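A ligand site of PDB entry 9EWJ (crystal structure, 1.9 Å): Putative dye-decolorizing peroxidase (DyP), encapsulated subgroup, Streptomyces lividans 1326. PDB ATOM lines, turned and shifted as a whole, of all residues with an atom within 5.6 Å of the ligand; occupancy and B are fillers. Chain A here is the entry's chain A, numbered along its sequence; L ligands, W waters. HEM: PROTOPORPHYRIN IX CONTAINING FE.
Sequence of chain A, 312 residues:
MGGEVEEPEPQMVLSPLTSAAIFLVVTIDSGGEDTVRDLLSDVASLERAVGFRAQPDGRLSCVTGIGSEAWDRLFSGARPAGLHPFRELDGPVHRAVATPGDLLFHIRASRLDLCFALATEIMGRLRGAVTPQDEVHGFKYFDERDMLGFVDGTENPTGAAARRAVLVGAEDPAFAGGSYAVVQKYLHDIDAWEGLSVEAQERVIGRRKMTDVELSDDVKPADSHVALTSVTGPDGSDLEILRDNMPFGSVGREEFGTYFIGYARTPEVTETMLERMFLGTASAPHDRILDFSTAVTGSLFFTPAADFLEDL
The side-chain hydroxyl of Ser 230 lies within hydrogen-bond range of an oxygen (O1D) of the ligand (3.5 Å). O1A of the ligand is in hydrogen-bond range of N of Thr 154, at 3.3 Å. The backbone NH (N) of Glu 155 is in hydrogen-bond range of an oxygen (O2A) of the ligand. An oxygen (O1A) of the ligand lies within salt-bridge range of the guanidinium group (NH2) of Arg 243 (3.0 Å). An iron atom (FE) of the ligand is bound by a ring nitrogen (NE2) of His 225, 2.0 Å away. An oxygen (O1A) of the ligand is in hydrogen-bond range of the backbone NH (N) of Gly 153.
O of Gln 184 sits at hydrogen-bond distance from N of Phe 260 (2.9 Å). A ring nitrogen (NE2) of His 188 lies within hydrogen-bond range of the side-chain hydroxyl (OG1) of Thr 258, at 2.8 Å. O of Ile 205 lies within hydrogen-bond range of N of His 225 (3.4 Å). O of Arg 243 sits at hydrogen-bond distance from ND2 of Asn 156, at 2.9 Å. OG1 of Thr 154 sits at hydrogen-bond distance from OD2 of Asp 212. O of Thr 258 sits at hydrogen-bond distance from N of Tyr 186. The side-chain carboxylate of Asp 152 lies within salt-bridge range of the guanidinium group of Arg 243 (3.8 Å). The guanidinium group of Arg 207 is in salt-bridge range of the side-chain carboxylate of Asp 212 (2.8 Å).
Asp 146 touches the ligand. Leu 148 touches the ligand (CD1 to CMB, 3.9 Å). Phe 150 touches the ligand (CB to CMA, 3.7 Å). O of Val 151 touches CMA of the ligand (3.3 Å). Asp 152 touches the ligand. Gln 184 touches the ligand. CG of Tyr 186 touches CBB of the ligand, 3.5 Å away. CD of Arg 207 touches CAA of the ligand, at 3.5 Å. Thr 229 touches the ligand (OG1 to C2D, 3.4 Å). Asn 245 touches the ligand. Thr 258 touches the ligand (OG1 to CMB, 3.7 Å). Phe 260 touches the ligand. Thr 270 touches the ligand. Met 273 touches the ligand. Leu 274 touches the ligand (CG to CBC, 3.9 Å). SD of Met 277 touches C2C of the ligand, 3.7 Å away. Ile 289 touches the ligand.
Water W1 lies within hydrogen-bond range of O2D of the ligand (2.8 Å) and NH1 of Arg 207 (3.1 Å). Water W2 lies within hydrogen-bond range of O of Thr 229 (2.8 Å) and O1D of the ligand (3.0 Å).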
ATOM      1  N   ASP A 146      -4.343  -1.554  35.143  1.00  0.00           N
ATOM      2  CA  ASP A 146      -5.119  -2.219  36.161  1.00  0.00           C
ATOM      3  C   ASP A 146      -4.158  -2.971  37.057  1.00  0.00           C
ATOM      4  O   ASP A 146      -2.948  -2.912  36.926  1.00  0.00           O
ATOM      5  CB  ASP A 146      -6.233  -3.050  35.535  1.00  0.00           C
ATOM      6  CG  ASP A 146      -5.780  -4.156  34.598  1.00  0.00           C
ATOM      7  OD1 ASP A 146      -4.651  -4.619  34.808  1.00  0.00           O
ATOM      8  OD2 ASP A 146      -6.528  -4.409  33.601  1.00  0.00           O
ATOM      9  N   LEU A 148      -3.674  -6.095  37.242  1.00  0.00           N
ATOM     10  CA  LEU A 148      -2.858  -7.127  36.612  1.00  0.00           C
ATOM     11  C   LEU A 148      -1.683  -6.552  35.857  1.00  0.00           C
ATOM     12  O   LEU A 148      -0.911  -7.269  35.265  1.00  0.00           O
ATOM     13  CB  LEU A 148      -3.788  -7.864  35.659  1.00  0.00           C
ATOM     14  CG  LEU A 148      -5.060  -8.478  36.256  1.00  0.00           C
ATOM     15  CD1 LEU A 148      -5.882  -9.116  35.140  1.00  0.00           C
ATOM     16  CD2 LEU A 148      -4.688  -9.506  37.327  1.00  0.00           C
ATOM     17  N   PHE A 150      -1.801  -4.463  33.148  1.00  0.00           N
ATOM     18  CA  PHE A 150      -2.088  -4.167  31.760  1.00  0.00           C
ATOM     19  C   PHE A 150      -2.838  -2.838  31.634  1.00  0.00           C
ATOM     20  O   PHE A 150      -3.591  -2.476  32.526  1.00  0.00           O
ATOM     21  CB  PHE A 150      -2.863  -5.330  31.154  1.00  0.00           C
ATOM     22  CG  PHE A 150      -1.943  -6.468  30.765  1.00  0.00           C
ATOM     23  CD1 PHE A 150      -1.446  -7.311  31.724  1.00  0.00           C
ATOM     24  CD2 PHE A 150      -1.679  -6.773  29.462  1.00  0.00           C
ATOM     25  CE1 PHE A 150      -0.677  -8.395  31.378  1.00  0.00           C
ATOM     26  CE2 PHE A 150      -0.897  -7.861  29.118  1.00  0.00           C
ATOM     27  CZ  PHE A 150      -0.380  -8.652  30.074  1.00  0.00           C
ATOM     28  N   VAL A 151      -2.587  -2.119  30.529  1.00  0.00           N
ATOM     29  CA  VAL A 151      -3.332  -0.899  30.215  1.00  0.00           C
ATOM     30  C   VAL A 151      -4.786  -1.307  29.972  1.00  0.00           C
ATOM     31  O   VAL A 151      -5.063  -2.266  29.230  1.00  0.00           O
ATOM     32  CB  VAL A 151      -2.762  -0.129  28.982  1.00  0.00           C
ATOM     33  CG1 VAL A 151      -3.589   1.123  28.708  1.00  0.00           C
ATOM     34  CG2 VAL A 151      -1.270   0.166  29.090  1.00  0.00           C
ATOM     35  N   ASP A 152      -5.706  -0.523  30.536  1.00  0.00           N
ATOM     36  CA  ASP A 152      -7.106  -0.872  30.611  1.00  0.00           C
ATOM     37  C   ASP A 152      -7.876   0.344  30.122  1.00  0.00           C
ATOM     38  O   ASP A 152      -7.823   1.419  30.754  1.00  0.00           O
ATOM     39  CB  ASP A 152      -7.427  -1.316  32.054  1.00  0.00           C
ATOM     40  CG  ASP A 152      -8.762  -2.014  32.315  1.00  0.00           C
ATOM     41  OD1 ASP A 152      -9.766  -1.471  31.759  1.00  0.00           O
ATOM     42  OD2 ASP A 152      -8.798  -3.063  33.143  1.00  0.00           O
ATOM     43  N   GLY A 153      -8.599   0.165  29.016  1.00  0.00           N
ATOM     44  CA  GLY A 153      -9.350   1.244  28.381  1.00  0.00           C
ATOM     45  C   GLY A 153      -9.090   1.402  26.866  1.00  0.00           C
ATOM     46  O   GLY A 153      -9.870   2.047  26.238  1.00  0.00           O
ATOM     47  N   THR A 154      -8.060   0.778  26.277  1.00  0.00           N
ATOM     48  CA  THR A 154      -7.453   1.194  25.031  1.00  0.00           C
ATOM     49  C   THR A 154      -8.429   1.094  23.880  1.00  0.00           C
ATOM     50  O   THR A 154      -8.536   1.984  23.061  1.00  0.00           O
ATOM     51  CB  THR A 154      -6.286   0.261  24.764  1.00  0.00           C
ATOM     52  OG1 THR A 154      -5.443   0.274  25.925  1.00  0.00           O
ATOM     53  CG2 THR A 154      -5.522   0.675  23.507  1.00  0.00           C
ATOM     54  N   GLU A 155      -9.180   0.003  23.831  1.00  0.00           N
ATOM     55  CA  GLU A 155     -10.154  -0.223  22.774  1.00  0.00           C
ATOM     56  C   GLU A 155     -11.561   0.274  23.067  1.00  0.00           C
ATOM     57  O   GLU A 155     -12.465   0.002  22.311  1.00  0.00           O
ATOM     58  CB  GLU A 155     -10.131  -1.685  22.343  1.00  0.00           C
ATOM     59  CG  GLU A 155      -8.857  -2.025  21.535  1.00  0.00           C
ATOM     60  CD  GLU A 155      -8.673  -1.246  20.247  1.00  0.00           C
ATOM     61  OE1 GLU A 155      -9.617  -1.341  19.492  1.00  0.00           O
ATOM     62  OE2 GLU A 155      -7.717  -0.541  20.001  1.00  0.00           O
ATOM     63  N   ASN A 156     -11.735   1.141  24.065  1.00  0.00           N
ATOM     64  CA  ASN A 156     -13.045   1.741  24.254  1.00  0.00           C
ATOM     65  C   ASN A 156     -13.433   2.558  23.052  1.00  0.00           C
ATOM     66  O   ASN A 156     -12.605   3.244  22.501  1.00  0.00           O
ATOM     67  CB  ASN A 156     -13.099   2.669  25.429  1.00  0.00           C
ATOM     68  CG  ASN A 156     -13.575   1.971  26.685  1.00  0.00           C
ATOM     69  OD1 ASN A 156     -14.408   1.042  26.606  1.00  0.00           O
ATOM     70  ND2 ASN A 156     -13.002   2.374  27.805  1.00  0.00           N
ATOM     71  N   GLN A 184     -19.641  -5.390  38.033  1.00  0.00           N
ATOM     72  CA  GLN A 184     -19.126  -6.527  38.741  1.00  0.00           C
ATOM     73  C   GLN A 184     -17.867  -6.134  39.527  1.00  0.00           C
ATOM     74  O   GLN A 184     -16.921  -5.583  38.969  1.00  0.00           O
ATOM     75  CB  GLN A 184     -18.753  -7.619  37.772  1.00  0.00           C
ATOM     76  CG  GLN A 184     -19.891  -8.239  37.000  1.00  0.00           C
ATOM     77  CD  GLN A 184     -19.333  -9.318  36.122  1.00  0.00           C
ATOM     78  OE1 GLN A 184     -18.541  -9.015  35.227  1.00  0.00           O
ATOM     79  NE2 GLN A 184     -19.613 -10.555  36.507  1.00  0.00           N
ATOM     80  N   TYR A 186     -14.551  -7.493  40.957  1.00  0.00           N
ATOM     81  CA  TYR A 186     -13.668  -8.641  40.812  1.00  0.00           C
ATOM     82  C   TYR A 186     -12.506  -8.537  41.787  1.00  0.00           C
ATOM     83  O   TYR A 186     -11.912  -7.469  41.924  1.00  0.00           O
ATOM     84  CB  TYR A 186     -13.012  -8.717  39.450  1.00  0.00           C
ATOM     85  CG  TYR A 186     -13.947  -9.256  38.385  1.00  0.00           C
ATOM     86  CD1 TYR A 186     -14.039 -10.609  38.174  1.00  0.00           C
ATOM     87  CD2 TYR A 186     -14.719  -8.369  37.630  1.00  0.00           C
ATOM     88  CE1 TYR A 186     -14.836 -11.083  37.163  1.00  0.00           C
ATOM     89  CE2 TYR A 186     -15.596  -8.849  36.680  1.00  0.00           C
ATOM     90  CZ  TYR A 186     -15.636 -10.216  36.418  1.00  0.00           C
ATOM     91  OH  TYR A 186     -16.457 -10.665  35.408  1.00  0.00           O
ATOM     92  N   HIS A 188      -8.661 -10.240  42.422  1.00  0.00           N
ATOM     93  CA  HIS A 188      -7.638 -10.987  41.721  1.00  0.00           C
ATOM     94  C   HIS A 188      -6.764 -11.752  42.704  1.00  0.00           C
ATOM     95  O   HIS A 188      -6.474 -11.259  43.790  1.00  0.00           O
ATOM     96  CB  HIS A 188      -6.754 -10.036  40.948  1.00  0.00           C
ATOM     97  CG  HIS A 188      -7.526  -9.270  39.940  1.00  0.00           C
ATOM     98  ND1 HIS A 188      -8.049  -9.904  38.852  1.00  0.00           N
ATOM     99  CD2 HIS A 188      -7.812  -7.962  39.803  1.00  0.00           C
ATOM    100  CE1 HIS A 188      -8.631  -8.995  38.063  1.00  0.00           C
ATOM    101  NE2 HIS A 188      -8.497  -7.793  38.622  1.00  0.00           N
ATOM    102  N   ILE A 205      -4.345 -12.128  28.264  1.00  0.00           N
ATOM    103  CA  ILE A 205      -5.075 -10.919  27.974  1.00  0.00           C
ATOM    104  C   ILE A 205      -5.306 -10.805  26.459  1.00  0.00           C
ATOM    105  O   ILE A 205      -6.403 -10.473  26.047  1.00  0.00           O
ATOM    106  CB  ILE A 205      -4.296  -9.703  28.512  1.00  0.00           C
ATOM    107  CG1 ILE A 205      -4.132  -9.753  29.996  1.00  0.00           C
ATOM    108  CG2 ILE A 205      -4.907  -8.362  28.078  1.00  0.00           C
ATOM    109  CD1 ILE A 205      -5.438  -9.648  30.723  1.00  0.00           C
ATOM    110  N   ARG A 207      -2.893  -8.932  24.531  1.00  0.00           N
ATOM    111  CA  ARG A 207      -2.128  -7.776  24.109  1.00  0.00           C
ATOM    112  C   ARG A 207      -0.767  -7.825  24.791  1.00  0.00           C
ATOM    113  O   ARG A 207      -0.570  -8.530  25.746  1.00  0.00           O
ATOM    114  CB  ARG A 207      -2.845  -6.503  24.567  1.00  0.00           C
ATOM    115  CG  ARG A 207      -4.305  -6.443  24.164  1.00  0.00           C
ATOM    116  CD  ARG A 207      -4.935  -5.125  24.537  1.00  0.00           C
ATOM    117  NE  ARG A 207      -4.417  -3.941  23.830  1.00  0.00           N
ATOM    118  CZ  ARG A 207      -4.841  -3.461  22.668  1.00  0.00           C
ATOM    119  NH1 ARG A 207      -5.865  -3.969  22.049  1.00  0.00           N
ATOM    120  NH2 ARG A 207      -4.333  -2.394  22.130  1.00  0.00           N
ATOM    121  N   ASP A 212       1.260  -2.351  25.034  1.00  0.00           N
ATOM    122  CA  ASP A 212      -0.173  -2.349  24.766  1.00  0.00           C
ATOM    123  C   ASP A 212      -0.493  -2.550  23.284  1.00  0.00           C
ATOM    124  O   ASP A 212      -1.533  -2.147  22.816  1.00  0.00           O
ATOM    125  CB  ASP A 212      -0.869  -1.095  25.240  1.00  0.00           C
ATOM    126  CG  ASP A 212      -2.377  -1.201  25.475  1.00  0.00           C
ATOM    127  OD1 ASP A 212      -2.924  -2.375  25.640  1.00  0.00           O
ATOM    128  OD2 ASP A 212      -2.982  -0.106  25.535  1.00  0.00           O
ATOM    129  N   GLU A 214      -1.860  -4.962  20.401  1.00  0.00           N
ATOM    130  CA  GLU A 214      -2.601  -6.209  20.304  1.00  0.00           C
ATOM    131  C   GLU A 214      -1.738  -7.325  19.709  1.00  0.00           C
ATOM    132  O   GLU A 214      -0.949  -7.074  18.844  1.00  0.00           O
ATOM    133  CB  GLU A 214      -3.827  -5.885  19.454  1.00  0.00           C
ATOM    134  CG  GLU A 214      -4.790  -7.054  19.266  1.00  0.00           C
ATOM    135  CD  GLU A 214      -6.141  -6.579  18.773  1.00  0.00           C
ATOM    136  OE1 GLU A 214      -6.481  -5.393  18.580  1.00  0.00           O
ATOM    137  OE2 GLU A 214      -6.906  -7.491  18.672  1.00  0.00           O
ATOM    138  N   HIS A 225      -8.710 -12.879  26.673  1.00  0.00           N
ATOM    139  CA  HIS A 225      -9.776 -11.982  27.062  1.00  0.00           C
ATOM    140  C   HIS A 225     -10.262 -11.163  25.872  1.00  0.00           C
ATOM    141  O   HIS A 225     -11.486 -10.972  25.667  1.00  0.00           O
ATOM    142  CB  HIS A 225      -9.314 -11.130  28.233  1.00  0.00           C
ATOM    143  CG  HIS A 225     -10.316 -10.149  28.693  1.00  0.00           C
ATOM    144  ND1 HIS A 225     -11.521 -10.532  29.198  1.00  0.00           N
ATOM    145  CD2 HIS A 225     -10.236  -8.821  28.826  1.00  0.00           C
ATOM    146  CE1 HIS A 225     -12.173  -9.434  29.602  1.00  0.00           C
ATOM    147  NE2 HIS A 225     -11.405  -8.383  29.371  1.00  0.00           N
ATOM    148  N   VAL A 226      -9.297 -10.683  25.096  1.00  0.00           N
ATOM    149  CA  VAL A 226      -9.607  -9.858  23.962  1.00  0.00           C
ATOM    150  C   VAL A 226     -10.300 -10.677  22.876  1.00  0.00           C
ATOM    151  O   VAL A 226     -11.129 -10.186  22.124  1.00  0.00           O
ATOM    152  CB  VAL A 226      -8.305  -9.193  23.456  1.00  0.00           C
ATOM    153  CG1 VAL A 226      -8.439  -8.805  21.997  1.00  0.00           C
ATOM    154  CG2 VAL A 226      -7.955  -7.986  24.347  1.00  0.00           C
ATOM    155  N   THR A 229     -14.045 -11.215  24.115  1.00  0.00           N
ATOM    156  CA  THR A 229     -14.883 -10.032  24.259  1.00  0.00           C
ATOM    157  C   THR A 229     -14.949  -9.235  22.947  1.00  0.00           C
ATOM    158  O   THR A 229     -15.459  -8.142  22.933  1.00  0.00           O
ATOM    159  CB  THR A 229     -14.382  -9.166  25.398  1.00  0.00           C
ATOM    160  OG1 THR A 229     -13.054  -8.722  25.133  1.00  0.00           O
ATOM    161  CG2 THR A 229     -14.473  -9.883  26.743  1.00  0.00           C
ATOM    162  N   SER A 230     -14.425  -9.767  21.848  1.00  0.00           N
ATOM    163  CA  SER A 230     -14.655  -9.236  20.525  1.00  0.00           C
ATOM    164  C   SER A 230     -15.856  -9.952  19.915  1.00  0.00           C
ATOM    165  O   SER A 230     -15.871 -11.163  19.817  1.00  0.00           O
ATOM    166  CB  SER A 230     -13.469  -9.450  19.637  1.00  0.00           C
ATOM    167  OG  SER A 230     -12.426  -8.643  20.147  1.00  0.00           O
ATOM    168  N   ILE A 241     -18.993  -1.898  23.833  1.00  0.00           N
ATOM    169  CA  ILE A 241     -19.422  -1.278  25.073  1.00  0.00           C
ATOM    170  C   ILE A 241     -18.420  -0.223  25.527  1.00  0.00           C
ATOM    171  O   ILE A 241     -17.309  -0.161  25.044  1.00  0.00           O
ATOM    172  CB  ILE A 241     -19.653  -2.305  26.196  1.00  0.00           C
ATOM    173  CG1 ILE A 241     -18.403  -2.908  26.710  1.00  0.00           C
ATOM    174  CG2 ILE A 241     -20.610  -3.382  25.717  1.00  0.00           C
ATOM    175  CD1 ILE A 241     -18.657  -3.823  27.896  1.00  0.00           C
ATOM    176  N   ARG A 243     -16.372   0.931  28.810  1.00  0.00           N
ATOM    177  CA  ARG A 243     -15.942   0.463  30.098  1.00  0.00           C
ATOM    178  C   ARG A 243     -15.209   1.583  30.824  1.00  0.00           C
ATOM    179  O   ARG A 243     -14.599   2.407  30.193  1.00  0.00           O
ATOM    180  CB  ARG A 243     -14.989  -0.725  30.007  1.00  0.00           C
ATOM    181  CG  ARG A 243     -15.606  -1.919  29.351  1.00  0.00           C
ATOM    182  CD  ARG A 243     -14.582  -2.962  29.039  1.00  0.00           C
ATOM    183  NE  ARG A 243     -13.893  -2.541  27.832  1.00  0.00           N
ATOM    184  CZ  ARG A 243     -12.573  -2.300  27.773  1.00  0.00           C
ATOM    185  NH1 ARG A 243     -11.802  -2.646  28.799  1.00  0.00           N
ATOM    186  NH2 ARG A 243     -12.017  -1.753  26.679  1.00  0.00           N
ATOM    187  N   ASN A 245     -13.290   0.646  33.992  1.00  0.00           N
ATOM    188  CA  ASN A 245     -12.778  -0.170  35.091  1.00  0.00           C
ATOM    189  C   ASN A 245     -11.852   0.644  36.004  1.00  0.00           C
ATOM    190  O   ASN A 245     -11.042   1.438  35.523  1.00  0.00           O
ATOM    191  CB  ASN A 245     -11.986  -1.371  34.567  1.00  0.00           C
ATOM    192  CG  ASN A 245     -12.837  -2.265  33.698  1.00  0.00           C
ATOM    193  OD1 ASN A 245     -14.088  -2.126  33.600  1.00  0.00           O
ATOM    194  ND2 ASN A 245     -12.160  -3.188  33.001  1.00  0.00           N
ATOM    195  N   THR A 258     -10.434  -5.193  40.594  1.00  0.00           N
ATOM    196  CA  THR A 258     -10.882  -4.379  39.466  1.00  0.00           C
ATOM    197  C   THR A 258     -12.376  -4.223  39.641  1.00  0.00           C
ATOM    198  O   THR A 258     -13.077  -5.201  39.774  1.00  0.00           O
ATOM    199  CB  THR A 258     -10.494  -5.059  38.137  1.00  0.00           C
ATOM    200  OG1 THR A 258      -9.068  -5.103  37.914  1.00  0.00           O
ATOM    201  CG2 THR A 258     -11.228  -4.403  36.957  1.00  0.00           C
ATOM    202  N   PHE A 260     -15.451  -3.497  37.637  1.00  0.00           N
ATOM    203  CA  PHE A 260     -15.853  -3.452  36.262  1.00  0.00           C
ATOM    204  C   PHE A 260     -17.179  -2.693  36.165  1.00  0.00           C
ATOM    205  O   PHE A 260     -18.111  -2.983  36.927  1.00  0.00           O
ATOM    206  CB  PHE A 260     -16.035  -4.867  35.729  1.00  0.00           C
ATOM    207  CG  PHE A 260     -16.726  -4.866  34.379  1.00  0.00           C
ATOM    208  CD1 PHE A 260     -16.000  -4.643  33.240  1.00  0.00           C
ATOM    209  CD2 PHE A 260     -18.071  -5.078  34.265  1.00  0.00           C
ATOM    210  CE1 PHE A 260     -16.610  -4.639  32.003  1.00  0.00           C
ATOM    211  CE2 PHE A 260     -18.665  -5.037  33.034  1.00  0.00           C
ATOM    212  CZ  PHE A 260     -17.933  -4.839  31.905  1.00  0.00           C
ATOM    213  N   THR A 270     -23.562  -6.606  26.384  1.00  0.00           N
ATOM    214  CA  THR A 270     -22.782  -6.924  27.579  1.00  0.00           C
ATOM    215  C   THR A 270     -22.984  -8.358  28.006  1.00  0.00           C
ATOM    216  O   THR A 270     -22.023  -9.025  28.372  1.00  0.00           O
ATOM    217  CB  THR A 270     -23.152  -5.967  28.701  1.00  0.00           C
ATOM    218  OG1 THR A 270     -23.066  -4.604  28.292  1.00  0.00           O
ATOM    219  CG2 THR A 270     -22.140  -6.040  29.807  1.00  0.00           C
ATOM    220  N   MET A 273     -21.056 -10.939  25.847  1.00  0.00           N
ATOM    221  CA  MET A 273     -19.656 -10.952  26.232  1.00  0.00           C
ATOM    222  C   MET A 273     -19.503 -11.785  27.511  1.00  0.00           C
ATOM    223  O   MET A 273     -18.600 -12.620  27.641  1.00  0.00           O
ATOM    224  CB  MET A 273     -19.184  -9.517  26.453  1.00  0.00           C
ATOM    225  CG  MET A 273     -18.973  -8.720  25.193  1.00  0.00           C
ATOM    226  SD  MET A 273     -18.638  -6.982  25.568  1.00  0.00           S
ATOM    227  CE  MET A 273     -18.492  -6.300  23.910  1.00  0.00           C
ATOM    228  N   LEU A 274     -20.376 -11.531  28.470  1.00  0.00           N
ATOM    229  CA  LEU A 274     -20.312 -12.267  29.723  1.00  0.00           C
ATOM    230  C   LEU A 274     -20.488 -13.779  29.521  1.00  0.00           C
ATOM    231  O   LEU A 274     -19.825 -14.569  30.197  1.00  0.00           O
ATOM    232  CB  LEU A 274     -21.366 -11.722  30.669  1.00  0.00           C
ATOM    233  CG  LEU A 274     -21.013 -10.454  31.434  1.00  0.00           C
ATOM    234  CD1 LEU A 274     -22.182  -9.846  32.216  1.00  0.00           C
ATOM    235  CD2 LEU A 274     -19.925 -10.809  32.420  1.00  0.00           C
ATOM    236  N   MET A 277     -17.430 -15.264  28.218  1.00  0.00           N
ATOM    237  CA  MET A 277     -16.354 -15.312  29.181  1.00  0.00           C
ATOM    238  C   MET A 277     -16.604 -16.472  30.133  1.00  0.00           C
ATOM    239  O   MET A 277     -15.681 -17.213  30.453  1.00  0.00           O
ATOM    240  CB  MET A 277     -16.233 -14.002  29.971  1.00  0.00           C
ATOM    241  CG  MET A 277     -15.696 -12.806  29.181  1.00  0.00           C
ATOM    242  SD  MET A 277     -15.861 -11.302  30.184  1.00  0.00           S
ATOM    243  CE  MET A 277     -14.729 -11.711  31.508  1.00  0.00           C
ATOM    244  N   ILE A 289      -8.831 -14.925  31.876  1.00  0.00           N
ATOM    245  CA  ILE A 289      -8.670 -13.924  32.909  1.00  0.00           C
ATOM    246  C   ILE A 289      -9.428 -14.364  34.176  1.00  0.00           C
ATOM    247  O   ILE A 289      -9.085 -13.924  35.269  1.00  0.00           O
ATOM    248  CB  ILE A 289      -9.149 -12.559  32.365  1.00  0.00           C
ATOM    249  CG1 ILE A 289      -8.497 -11.419  33.075  1.00  0.00           C
ATOM    250  CG2 ILE A 289     -10.652 -12.394  32.488  1.00  0.00           C
ATOM    251  CD1 ILE A 289      -8.866 -10.029  32.560  1.00  0.00           C
ATOM    252  N   LEU A 290     -10.499 -15.191  34.040  1.00  0.00           N
ATOM    253  CA  LEU A 290     -11.274 -15.652  35.183  1.00  0.00           C
ATOM    254  C   LEU A 290     -10.522 -16.704  36.030  1.00  0.00           C
ATOM    255  O   LEU A 290     -10.864 -16.968  37.161  1.00  0.00           O
ATOM    256  CB  LEU A 290     -12.611 -16.205  34.703  1.00  0.00           C
ATOM    257  CG  LEU A 290     -13.495 -15.188  34.000  1.00  0.00           C
ATOM    258  CD1 LEU A 290     -14.728 -15.969  33.546  1.00  0.00           C
ATOM    259  CD2 LEU A 290     -13.893 -14.092  34.873  1.00  0.00           C
ATOM    260  N   SER A 293      -9.387 -14.127  38.526  1.00  0.00           N
ATOM    261  CA  SER A 293     -10.311 -13.062  38.849  1.00  0.00           C
ATOM    262  C   SER A 293     -11.618 -13.738  39.291  1.00  0.00           C
ATOM    263  O   SER A 293     -12.198 -14.546  38.540  1.00  0.00           O
ATOM    264  CB  SER A 293     -10.531 -12.103  37.678  1.00  0.00           C
ATOM    265  OG  SER A 293      -9.336 -11.804  36.981  1.00  0.00           O
HETATM  266  CHA HEM L   1     -10.425  -5.305  27.040  1.00  0.00           C
HETATM  267  CHB HEM L   1      -9.009  -6.045  31.576  1.00  0.00           C
HETATM  268  CHC HEM L   1     -13.490  -7.660  32.714  1.00  0.00           C
HETATM  269  CHD HEM L   1     -14.879  -6.435  28.245  1.00  0.00           C
HETATM  270  C1A HEM L   1      -9.613  -5.377  28.184  1.00  0.00           C
HETATM  271  C2A HEM L   1      -8.220  -5.164  28.205  1.00  0.00           C
HETATM  272  C3A HEM L   1      -7.817  -5.332  29.500  1.00  0.00           C
HETATM  273  C4A HEM L   1      -8.938  -5.753  30.274  1.00  0.00           C
HETATM  274  CMA HEM L   1      -6.410  -5.127  30.000  1.00  0.00           C
HETATM  275  CAA HEM L   1      -7.340  -4.746  27.040  1.00  0.00           C
HETATM  276  CBA HEM L   1      -7.292  -3.202  26.883  1.00  0.00           C
HETATM  277  CGA HEM L   1      -8.581  -2.576  26.517  1.00  0.00           C
HETATM  278  O1A HEM L   1      -9.165  -2.032  27.482  1.00  0.00           O
HETATM  279  O2A HEM L   1      -8.972  -2.612  25.289  1.00  0.00           O
HETATM  280  C1B HEM L   1     -10.115  -6.514  32.295  1.00  0.00           C
HETATM  281  C2B HEM L   1     -10.066  -6.909  33.653  1.00  0.00           C
HETATM  282  C3B HEM L   1     -11.335  -7.299  34.017  1.00  0.00           C
HETATM  283  C4B HEM L   1     -12.159  -7.285  32.794  1.00  0.00           C
HETATM  284  CMB HEM L   1      -8.894  -6.739  34.649  1.00  0.00           C
HETATM  285  CAB HEM L   1     -11.585  -7.825  35.381  1.00  0.00           C
HETATM  286  CBB HEM L   1     -12.074  -9.046  35.464  1.00  0.00           C
HETATM  287  C1C HEM L   1     -14.293  -7.501  31.628  1.00  0.00           C
HETATM  288  C2C HEM L   1     -15.692  -7.868  31.494  1.00  0.00           C
HETATM  289  C3C HEM L   1     -16.064  -7.565  30.161  1.00  0.00           C
HETATM  290  C4C HEM L   1     -14.908  -6.989  29.545  1.00  0.00           C
HETATM  291  CMC HEM L   1     -16.579  -8.472  32.545  1.00  0.00           C
HETATM  292  CAC HEM L   1     -17.315  -7.633  29.384  1.00  0.00           C
HETATM  293  CBC HEM L   1     -18.471  -8.039  29.835  1.00  0.00           C
HETATM  294  C1D HEM L   1     -13.814  -5.957  27.555  1.00  0.00           C
HETATM  295  C2D HEM L   1     -13.927  -5.560  26.188  1.00  0.00           C
HETATM  296  C3D HEM L   1     -12.642  -5.272  25.807  1.00  0.00           C
HETATM  297  C4D HEM L   1     -11.812  -5.543  27.029  1.00  0.00           C
HETATM  298  CMD HEM L   1     -15.189  -5.429  25.365  1.00  0.00           C
HETATM  299  CAD HEM L   1     -12.112  -4.704  24.462  1.00  0.00           C
HETATM  300  CBD HEM L   1     -11.869  -5.869  23.392  1.00  0.00           C
HETATM  301  CGD HEM L   1     -11.467  -5.428  21.947  1.00  0.00           C
HETATM  302  O1D HEM L   1     -12.220  -5.274  20.979  1.00  0.00           O
HETATM  303  O2D HEM L   1     -10.299  -5.160  21.719  1.00  0.00           O
HETATM  304  NA  HEM L   1     -10.025  -5.783  29.461  1.00  0.00           N
HETATM  305  NB  HEM L   1     -11.354  -6.761  31.836  1.00  0.00           N
HETATM  306  NC  HEM L   1     -13.871  -6.953  30.468  1.00  0.00           N
HETATM  307  ND  HEM L   1     -12.563  -5.970  28.021  1.00  0.00           N
HETATM  308 FE   HEM L   1     -11.924  -6.452  29.800  1.00  0.00          FE
HETATM  309  O   HOH W   1      -8.361  -4.751  23.645  1.00  0.00           O
HETATM  310  O   HOH W   2     -15.004  -5.466  22.154  1.00  0.00           O
